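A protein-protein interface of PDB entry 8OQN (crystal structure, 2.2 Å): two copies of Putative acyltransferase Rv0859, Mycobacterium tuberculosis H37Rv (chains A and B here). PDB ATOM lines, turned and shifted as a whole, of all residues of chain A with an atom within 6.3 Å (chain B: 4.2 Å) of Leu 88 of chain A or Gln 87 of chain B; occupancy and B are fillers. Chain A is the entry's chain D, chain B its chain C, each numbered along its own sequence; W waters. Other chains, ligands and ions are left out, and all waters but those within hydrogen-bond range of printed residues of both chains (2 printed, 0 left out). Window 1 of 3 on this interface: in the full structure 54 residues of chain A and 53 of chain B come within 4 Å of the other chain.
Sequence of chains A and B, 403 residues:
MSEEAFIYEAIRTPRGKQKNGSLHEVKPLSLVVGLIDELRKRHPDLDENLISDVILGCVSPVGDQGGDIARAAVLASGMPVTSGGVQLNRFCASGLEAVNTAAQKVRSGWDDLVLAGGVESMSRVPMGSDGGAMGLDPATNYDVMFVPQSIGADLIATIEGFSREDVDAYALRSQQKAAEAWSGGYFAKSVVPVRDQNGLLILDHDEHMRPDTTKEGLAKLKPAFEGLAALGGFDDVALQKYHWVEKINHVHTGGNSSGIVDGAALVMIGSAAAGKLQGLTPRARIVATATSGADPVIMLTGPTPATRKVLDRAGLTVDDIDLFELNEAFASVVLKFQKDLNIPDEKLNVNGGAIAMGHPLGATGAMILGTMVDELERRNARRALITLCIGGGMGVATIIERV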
ATOM      1  N   ILE A  55     -10.757 -18.740  17.660  1.00  0.00           N
ATOM      2  CA  ILE A  55     -10.702 -17.344  17.237  1.00  0.00           C
ATOM      3  C   ILE A  55      -9.560 -16.665  17.978  1.00  0.00           C
ATOM      4  O   ILE A  55      -9.580 -16.576  19.211  1.00  0.00           O
ATOM      5  CB  ILE A  55     -12.035 -16.624  17.496  1.00  0.00           C
ATOM      6  CG1 ILE A  55     -13.192 -17.423  16.890  1.00  0.00           C
ATOM      7  CG2 ILE A  55     -11.994 -15.217  16.930  1.00  0.00           C
ATOM      8  CD1 ILE A  55     -14.563 -16.843  17.174  1.00  0.00           C
ATOM      9  N   LEU A  56      -8.571 -16.183  17.231  1.00  0.00           N
ATOM     10  CA  LEU A  56      -7.382 -15.563  17.803  1.00  0.00           C
ATOM     11  C   LEU A  56      -7.237 -14.138  17.295  1.00  0.00           C
ATOM     12  O   LEU A  56      -7.291 -13.897  16.083  1.00  0.00           O
ATOM     13  CB  LEU A  56      -6.123 -16.356  17.463  1.00  0.00           C
ATOM     14  CG  LEU A  56      -5.993 -17.761  18.045  1.00  0.00           C
ATOM     15  CD1 LEU A  56      -4.620 -18.326  17.711  1.00  0.00           C
ATOM     16  CD2 LEU A  56      -6.217 -17.743  19.546  1.00  0.00           C
ATOM     17  N   GLY A  57      -7.044 -13.201  18.221  1.00  0.00           N
ATOM     18  CA  GLY A  57      -6.672 -11.853  17.840  1.00  0.00           C
ATOM     19  C   GLY A  57      -5.178 -11.769  17.565  1.00  0.00           C
ATOM     20  O   GLY A  57      -4.360 -12.376  18.255  1.00  0.00           O
ATOM     21  N   CYS A  58      -4.830 -11.020  16.524  1.00  0.00           N
ATOM     22  CA  CYS A  58      -3.427 -10.834  16.165  1.00  0.00           C
ATOM     23  C   CYS A  58      -3.318  -9.561  15.346  1.00  0.00           C
ATOM     24  O   CYS A  58      -3.905  -9.468  14.263  1.00  0.00           O
ATOM     25  CB  CYS A  58      -2.892 -12.034  15.386  1.00  0.00           C
ATOM     26  SG  CYS A  58      -1.114 -11.977  15.095  1.00  0.00           S
ATOM     27  N   VAL A  59      -2.569  -8.587  15.863  1.00  0.00           N
ATOM     28  CA  VAL A  59      -2.545  -7.256  15.267  1.00  0.00           C
ATOM     29  C   VAL A  59      -1.571  -7.182  14.095  1.00  0.00           C
ATOM     30  O   VAL A  59      -1.794  -6.417  13.147  1.00  0.00           O
ATOM     31  CB  VAL A  59      -2.217  -6.217  16.353  1.00  0.00           C
ATOM     32  CG1 VAL A  59      -2.098  -4.826  15.761  1.00  0.00           C
ATOM     33  CG2 VAL A  59      -3.285  -6.247  17.427  1.00  0.00           C
ATOM     34  N   PRO A  61      -0.551  -9.822  11.699  1.00  0.00           N
ATOM     35  CA  PRO A  61      -0.600 -11.185  11.152  1.00  0.00           C
ATOM     36  C   PRO A  61       0.361 -11.362   9.984  1.00  0.00           C
ATOM     37  O   PRO A  61      -0.053 -11.435   8.823  1.00  0.00           O
ATOM     38  CB  PRO A  61      -2.063 -11.334  10.721  1.00  0.00           C
ATOM     39  CG  PRO A  61      -2.491  -9.947  10.402  1.00  0.00           C
ATOM     40  CD  PRO A  61      -1.735  -9.031  11.321  1.00  0.00           C
ATOM     41  N   VAL A  86      -9.771 -18.994  13.001  1.00  0.00           N
ATOM     42  CA  VAL A  86      -9.866 -17.725  12.288  1.00  0.00           C
ATOM     43  C   VAL A  86      -9.079 -16.665  13.050  1.00  0.00           C
ATOM     44  O   VAL A  86      -9.130 -16.599  14.283  1.00  0.00           O
ATOM     45  CB  VAL A  86     -11.338 -17.298  12.092  1.00  0.00           C
ATOM     46  CG1 VAL A  86     -12.093 -17.372  13.409  1.00  0.00           C
ATOM     47  CG2 VAL A  86     -11.427 -15.899  11.491  1.00  0.00           C
ATOM     48  N   GLN A  87      -8.343 -15.843  12.305  1.00  0.00           N
ATOM     49  CA  GLN A  87      -7.578 -14.726  12.841  1.00  0.00           C
ATOM     50  C   GLN A  87      -8.341 -13.428  12.611  1.00  0.00           C
ATOM     51  O   GLN A  87      -8.967 -13.248  11.564  1.00  0.00           O
ATOM     52  CB  GLN A  87      -6.198 -14.657  12.175  1.00  0.00           C
ATOM     53  CG  GLN A  87      -5.377 -13.412  12.500  1.00  0.00           C
ATOM     54  CD  GLN A  87      -5.592 -12.275  11.510  1.00  0.00           C
ATOM     55  OE1 GLN A  87      -5.705 -12.496  10.302  1.00  0.00           O
ATOM     56  NE2 GLN A  87      -5.652 -11.052  12.021  1.00  0.00           N
ATOM     57  N   LEU A  88      -8.293 -12.526  13.592  1.00  0.00           N
ATOM     58  CA  LEU A  88      -8.921 -11.220  13.441  1.00  0.00           C
ATOM     59  C   LEU A  88      -8.028 -10.139  14.035  1.00  0.00           C
ATOM     60  O   LEU A  88      -7.176 -10.401  14.889  1.00  0.00           O
ATOM     61  CB  LEU A  88     -10.322 -11.171  14.079  1.00  0.00           C
ATOM     62  CG  LEU A  88     -10.576 -11.390  15.576  1.00  0.00           C
ATOM     63  CD1 LEU A  88     -10.220 -10.176  16.425  1.00  0.00           C
ATOM     64  CD2 LEU A  88     -12.041 -11.742  15.782  1.00  0.00           C
ATOM     65  N   ASN A  89      -8.249  -8.908  13.572  1.00  0.00           N
ATOM     66  CA  ASN A  89      -7.463  -7.753  13.990  1.00  0.00           C
ATOM     67  C   ASN A  89      -8.396  -6.573  14.207  1.00  0.00           C
ATOM     68  O   ASN A  89      -9.027  -6.094  13.260  1.00  0.00           O
ATOM     69  CB  ASN A  89      -6.391  -7.408  12.946  1.00  0.00           C
ATOM     70  CG  ASN A  89      -5.635  -6.127  13.275  1.00  0.00           C
ATOM     71  OD1 ASN A  89      -5.635  -5.660  14.413  1.00  0.00           O
ATOM     72  ND2 ASN A  89      -4.979  -5.558  12.269  1.00  0.00           N
ATOM     73  N   ARG A  90      -8.488  -6.117  15.453  1.00  0.00           N
ATOM     74  CA  ARG A  90      -9.097  -4.832  15.794  1.00  0.00           C
ATOM     75  C   ARG A  90      -8.162  -4.051  16.710  1.00  0.00           C
ATOM     76  O   ARG A  90      -8.570  -3.475  17.721  1.00  0.00           O
ATOM     77  CB  ARG A  90     -10.469  -5.004  16.439  1.00  0.00           C
ATOM     78  CG  ARG A  90     -11.333  -3.750  16.343  1.00  0.00           C
ATOM     79  CD  ARG A  90     -12.344  -3.637  17.474  1.00  0.00           C
ATOM     80  NE  ARG A  90     -13.466  -4.554  17.314  1.00  0.00           N
ATOM     81  CZ  ARG A  90     -14.522  -4.316  16.549  1.00  0.00           C
ATOM     82  NH1 ARG A  90     -14.620  -3.211  15.830  1.00  0.00           N
ATOM     83  NH2 ARG A  90     -15.505  -5.212  16.503  1.00  0.00           N
ATOM     84  N   ALA A  93      -7.855  -4.158  20.965  1.00  0.00           N
ATOM     85  CA  ALA A  93      -8.960  -4.935  21.512  1.00  0.00           C
ATOM     86  C   ALA A  93      -9.118  -6.298  20.855  1.00  0.00           C
ATOM     87  O   ALA A  93     -10.113  -6.980  21.117  1.00  0.00           O
ATOM     88  CB  ALA A  93     -10.271  -4.161  21.382  1.00  0.00           C
ATOM     89  N   SER A  94      -8.161  -6.708  20.017  1.00  0.00           N
ATOM     90  CA  SER A  94      -8.318  -7.937  19.243  1.00  0.00           C
ATOM     91  C   SER A  94      -8.566  -9.144  20.141  1.00  0.00           C
ATOM     92  O   SER A  94      -9.397 -10.003  19.822  1.00  0.00           O
ATOM     93  CB  SER A  94      -7.086  -8.161  18.367  1.00  0.00           C
ATOM     94  OG  SER A  94      -6.900  -7.088  17.458  1.00  0.00           O
ATOM     95  N   GLY A  95      -7.859  -9.226  21.271  1.00  0.00           N
ATOM     96  CA  GLY A  95      -8.060 -10.345  22.177  1.00  0.00           C
ATOM     97  C   GLY A  95      -9.437 -10.349  22.811  1.00  0.00           C
ATOM     98  O   GLY A  95     -10.052 -11.407  22.976  1.00  0.00           O
ATOM     99  N   GLU A  97     -12.082  -8.706  21.461  1.00  0.00           N
ATOM    100  CA  GLU A  97     -13.014  -8.880  20.351  1.00  0.00           C
ATOM    101  C   GLU A  97     -13.174 -10.353  19.994  1.00  0.00           C
ATOM    102  O   GLU A  97     -14.277 -10.805  19.665  1.00  0.00           O
ATOM    103  CB  GLU A  97     -12.544  -8.079  19.138  1.00  0.00           C
ATOM    104  CG  GLU A  97     -13.427  -8.246  17.911  1.00  0.00           C
ATOM    105  CD  GLU A  97     -14.865  -7.829  18.172  1.00  0.00           C
ATOM    106  OE1 GLU A  97     -15.075  -6.755  18.775  1.00  0.00           O
ATOM    107  OE2 GLU A  97     -15.784  -8.581  17.782  1.00  0.00           O
ATOM    108  N   ALA A  98     -12.082 -11.121  20.061  1.00  0.00           N
ATOM    109  CA  ALA A  98     -12.176 -12.555  19.812  1.00  0.00           C
ATOM    110  C   ALA A  98     -13.073 -13.235  20.838  1.00  0.00           C
ATOM    111  O   ALA A  98     -13.886 -14.097  20.491  1.00  0.00           O
ATOM    112  CB  ALA A  98     -10.784 -13.184  19.817  1.00  0.00           C
ATOM    113  N   THR A 101     -16.702 -12.118  20.037  1.00  0.00           N
ATOM    114  CA  THR A 101     -17.216 -12.830  18.871  1.00  0.00           C
ATOM    115  C   THR A 101     -17.522 -14.283  19.212  1.00  0.00           C
ATOM    116  O   THR A 101     -18.514 -14.847  18.733  1.00  0.00           O
ATOM    117  CB  THR A 101     -16.215 -12.745  17.717  1.00  0.00           C
ATOM    118  OG1 THR A 101     -16.046 -11.375  17.331  1.00  0.00           O
ATOM    119  CG2 THR A 101     -16.703 -13.545  16.516  1.00  0.00           C
ATOM    120  N   LEU B  56     -14.556  -7.002   7.514  1.00  0.00           N
ATOM    121  CA  LEU B  56     -14.033  -7.300   6.187  1.00  0.00           C
ATOM    122  C   LEU B  56     -13.105  -8.503   6.251  1.00  0.00           C
ATOM    123  O   LEU B  56     -12.152  -8.514   7.037  1.00  0.00           O
ATOM    124  CB  LEU B  56     -13.277  -6.102   5.604  1.00  0.00           C
ATOM    125  CG  LEU B  56     -14.040  -4.811   5.304  1.00  0.00           C
ATOM    126  CD1 LEU B  56     -13.110  -3.805   4.652  1.00  0.00           C
ATOM    127  CD2 LEU B  56     -15.242  -5.078   4.412  1.00  0.00           C
ATOM    128  N   CYS B  58     -10.090 -10.661   4.686  1.00  0.00           N
ATOM    129  CA  CYS B  58      -8.900 -10.364   3.893  1.00  0.00           C
ATOM    130  C   CYS B  58      -7.852 -11.419   4.204  1.00  0.00           C
ATOM    131  O   CYS B  58      -7.463 -11.580   5.366  1.00  0.00           O
ATOM    132  CB  CYS B  58      -8.371  -8.960   4.195  1.00  0.00           C
ATOM    133  SG  CYS B  58      -7.020  -8.417   3.126  1.00  0.00           S
ATOM    134  N   PRO B  61      -3.524  -9.751   4.714  1.00  0.00           N
ATOM    135  CA  PRO B  61      -3.604  -8.402   5.318  1.00  0.00           C
ATOM    136  C   PRO B  61      -2.232  -7.777   5.555  1.00  0.00           C
ATOM    137  O   PRO B  61      -1.784  -7.563   6.684  1.00  0.00           O
ATOM    138  CB  PRO B  61      -4.360  -8.672   6.622  1.00  0.00           C
ATOM    139  CG  PRO B  61      -3.947 -10.053   7.004  1.00  0.00           C
ATOM    140  CD  PRO B  61      -3.726 -10.814   5.716  1.00  0.00           C
ATOM    141  N   ASP B  68      -5.565  -3.324   9.725  1.00  0.00           N
ATOM    142  CA  ASP B  68      -7.021  -3.302   9.861  1.00  0.00           C
ATOM    143  C   ASP B  68      -7.661  -2.436   8.778  1.00  0.00           C
ATOM    144  O   ASP B  68      -8.072  -1.302   9.045  1.00  0.00           O
ATOM    145  CB  ASP B  68      -7.428  -2.803  11.250  1.00  0.00           C
ATOM    146  CG  ASP B  68      -8.894  -3.043  11.551  1.00  0.00           C
ATOM    147  OD1 ASP B  68      -9.636  -3.479  10.644  1.00  0.00           O
ATOM    148  OD2 ASP B  68      -9.304  -2.816  12.705  1.00  0.00           O
ATOM    149  N   VAL B  86     -13.127  -4.258  11.770  1.00  0.00           N
ATOM    150  CA  VAL B  86     -12.309  -5.408  12.139  1.00  0.00           C
ATOM    151  C   VAL B  86     -12.007  -6.226  10.891  1.00  0.00           C
ATOM    152  O   VAL B  86     -12.898  -6.474  10.070  1.00  0.00           O
ATOM    153  CB  VAL B  86     -12.995  -6.278  13.214  1.00  0.00           C
ATOM    154  CG1 VAL B  86     -14.433  -6.566  12.828  1.00  0.00           C
ATOM    155  CG2 VAL B  86     -12.223  -7.575  13.437  1.00  0.00           C
ATOM    156  N   GLN B  87     -10.747  -6.620  10.738  1.00  0.00           N
ATOM    157  CA  GLN B  87     -10.303  -7.506   9.673  1.00  0.00           C
ATOM    158  C   GLN B  87     -10.245  -8.933  10.203  1.00  0.00           C
ATOM    159  O   GLN B  87      -9.880  -9.156  11.360  1.00  0.00           O
ATOM    160  CB  GLN B  87      -8.929  -7.070   9.151  1.00  0.00           C
ATOM    161  CG  GLN B  87      -8.256  -8.033   8.174  1.00  0.00           C
ATOM    162  CD  GLN B  87      -7.390  -9.077   8.865  1.00  0.00           C
ATOM    163  OE1 GLN B  87      -6.634  -8.764   9.783  1.00  0.00           O
ATOM    164  NE2 GLN B  87      -7.503 -10.326   8.423  1.00  0.00           N
ATOM    165  N   LEU B  88     -10.615  -9.898   9.362  1.00  0.00           N
ATOM    166  CA  LEU B  88     -10.505 -11.301   9.740  1.00  0.00           C
ATOM    167  C   LEU B  88     -10.025 -12.118   8.551  1.00  0.00           C
ATOM    168  O   LEU B  88     -10.165 -11.719   7.392  1.00  0.00           O
ATOM    169  CB  LEU B  88     -11.830 -11.864  10.286  1.00  0.00           C
ATOM    170  CG  LEU B  88     -13.101 -12.034   9.444  1.00  0.00           C
ATOM    171  CD1 LEU B  88     -13.071 -13.277   8.556  1.00  0.00           C
ATOM    172  CD2 LEU B  88     -14.311 -12.089  10.365  1.00  0.00           C
ATOM    173  N   ASN B  89      -9.458 -13.283   8.861  1.00  0.00           N
ATOM    174  CA  ASN B  89      -8.886 -14.173   7.854  1.00  0.00           C
ATOM    175  C   ASN B  89      -9.274 -15.605   8.194  1.00  0.00           C
ATOM    176  O   ASN B  89      -8.846 -16.137   9.222  1.00  0.00           O
ATOM    177  CB  ASN B  89      -7.366 -14.020   7.789  1.00  0.00           C
ATOM    178  CG  ASN B  89      -6.716 -15.029   6.861  1.00  0.00           C
ATOM    179  OD1 ASN B  89      -7.361 -15.577   5.966  1.00  0.00           O
ATOM    180  ND2 ASN B  89      -5.427 -15.278   7.068  1.00  0.00           N
HETATM  181  O   HOH W   1      -5.089  -6.530   9.606  1.00  0.00           O
HETATM  182  O   HOH W   2      -3.869 -14.010   8.989  1.00  0.00           O
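Water W2 bridges OE1 of Gln 87 of chain A (2.7 Å) and ND2 of Asn 89 of chain B (2.8 Å).
Water W1 lies within hydrogen-bond range of the side-chain amide oxygen (OE1) of Gln 87 of chain B, the side-chain amide nitrogen (ND2) of Asn 89 of chain A and the backbone NH (N) of Asp 68 of chain B.
Of the printed residues of chain A, Asn 89 of chain B touches Val 86 (3.4 Å) and Gln 87 (2.7 Å).
Of the printed residues of chain B, Val 86 of chain A touches Asn 89.
Of the printed residues of chain A, Leu 88 of chain B touches Gln 87 (3.1 Å).
Leu 56 of chain A touches none of the printed residues of chain B.
The nearest residue of chain B that does not touch Leu 88 of chain A is Leu 88 of chain B (4.03 Å).
The nearest residue of chain A that does not touch Gln 87 of chain B is Pro 61 of chain A (4.4 Å).
The side-chain amide nitrogen (ND2) of Asn 89 of chain A sits close to the backbone NH (N) of Asp 68 of chain B (3.4 Å).
OE1 of Gln 87 of chain B lies within hydrogen-bond range of NE2 of Gln 87 of chain A (3.3 Å).
O of Gln 87 of chain B sits at hydrogen-bond distance from N of Asn 89 of chain A, at 2.8 Å.
The backbone carbonyl oxygen of Gln 87 of chain A sits at hydrogen-bond distance from the backbone NH of Asn 89 of chain B (2.7 Å).
The backbone carbonyl oxygen of Val 86 of chain B lies within hydrogen-bond range of the backbone NH of Leu 56 of chain B, at 3.1 Å.
NE2 of Gln 87 of chain B sits at hydrogen-bond distance from O of Cys 58 of chain B (3.3 Å).
The backbone NH (N) of Gln 87 of chain B lies within hydrogen-bond range of the side-chain carboxylate (OD1) of Asp 68 of chain B (3.3 Å).
O of Cys 58 of chain A sits at hydrogen-bond distance from NE2 of Gln 87 of chain A.
O of Leu 88 of chain A sits at hydrogen-bond distance from N of Cys 58 of chain A, at 2.9 Å.
NH2 of Arg 90 of chain A is in salt-bridge range of OE1 of Glu 97 of chain A (2.8 Å).
CG of Pro 61 of chain A touches CG of Pro 61 of chain B, at 3.7 Å.
Val 86 of chain A touches Asn 89 of chain B.
Gln 87 of chain A touches Leu 88 of chain B (O to CA, 3.1 Å).
CA of Leu 88 of chain A touches O of Gln 87 of chain B, at 3.1 Å.
Asn 89 of chain A touches Val 86 of chain B.
Asp 68 of chain B touches Arg 90 of chain A.
Hydrophobic or aromatic side chains of chain B that line the printed part of chain A: Pro 61, Val 86 and Leu 88.
Of the 17 printed residues of chain A, 6 touch a printed residue of chain B.
Hydrophobic or aromatic side chains of chain A within 4 Å of the printed part of chain B: Pro 61, Val 86 and Leu 88.
Among the printed residues, no Asp or Glu carboxylate lies within 4 Å of a Lys or Arg side-chain nitrogen of the other chain.
Pro 61 of chain B touches its own counterpart, Pro 61 of chain A.
Val 86 of chain A touches Asn 89 of chain B, and with the chains exchanged Asn 89 of chain A touches Val 86 of chain B.
Gln 87 of chain B touches its own counterpart, Gln 87 of chain A.
Gln 87 of chain A touches Leu 88 of chain B, and with the chains exchanged Leu 88 of chain A touches Gln 87 of chain B.
Positions printed for both chains: 56, 58, 61, 86, 87, 88 and 89.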
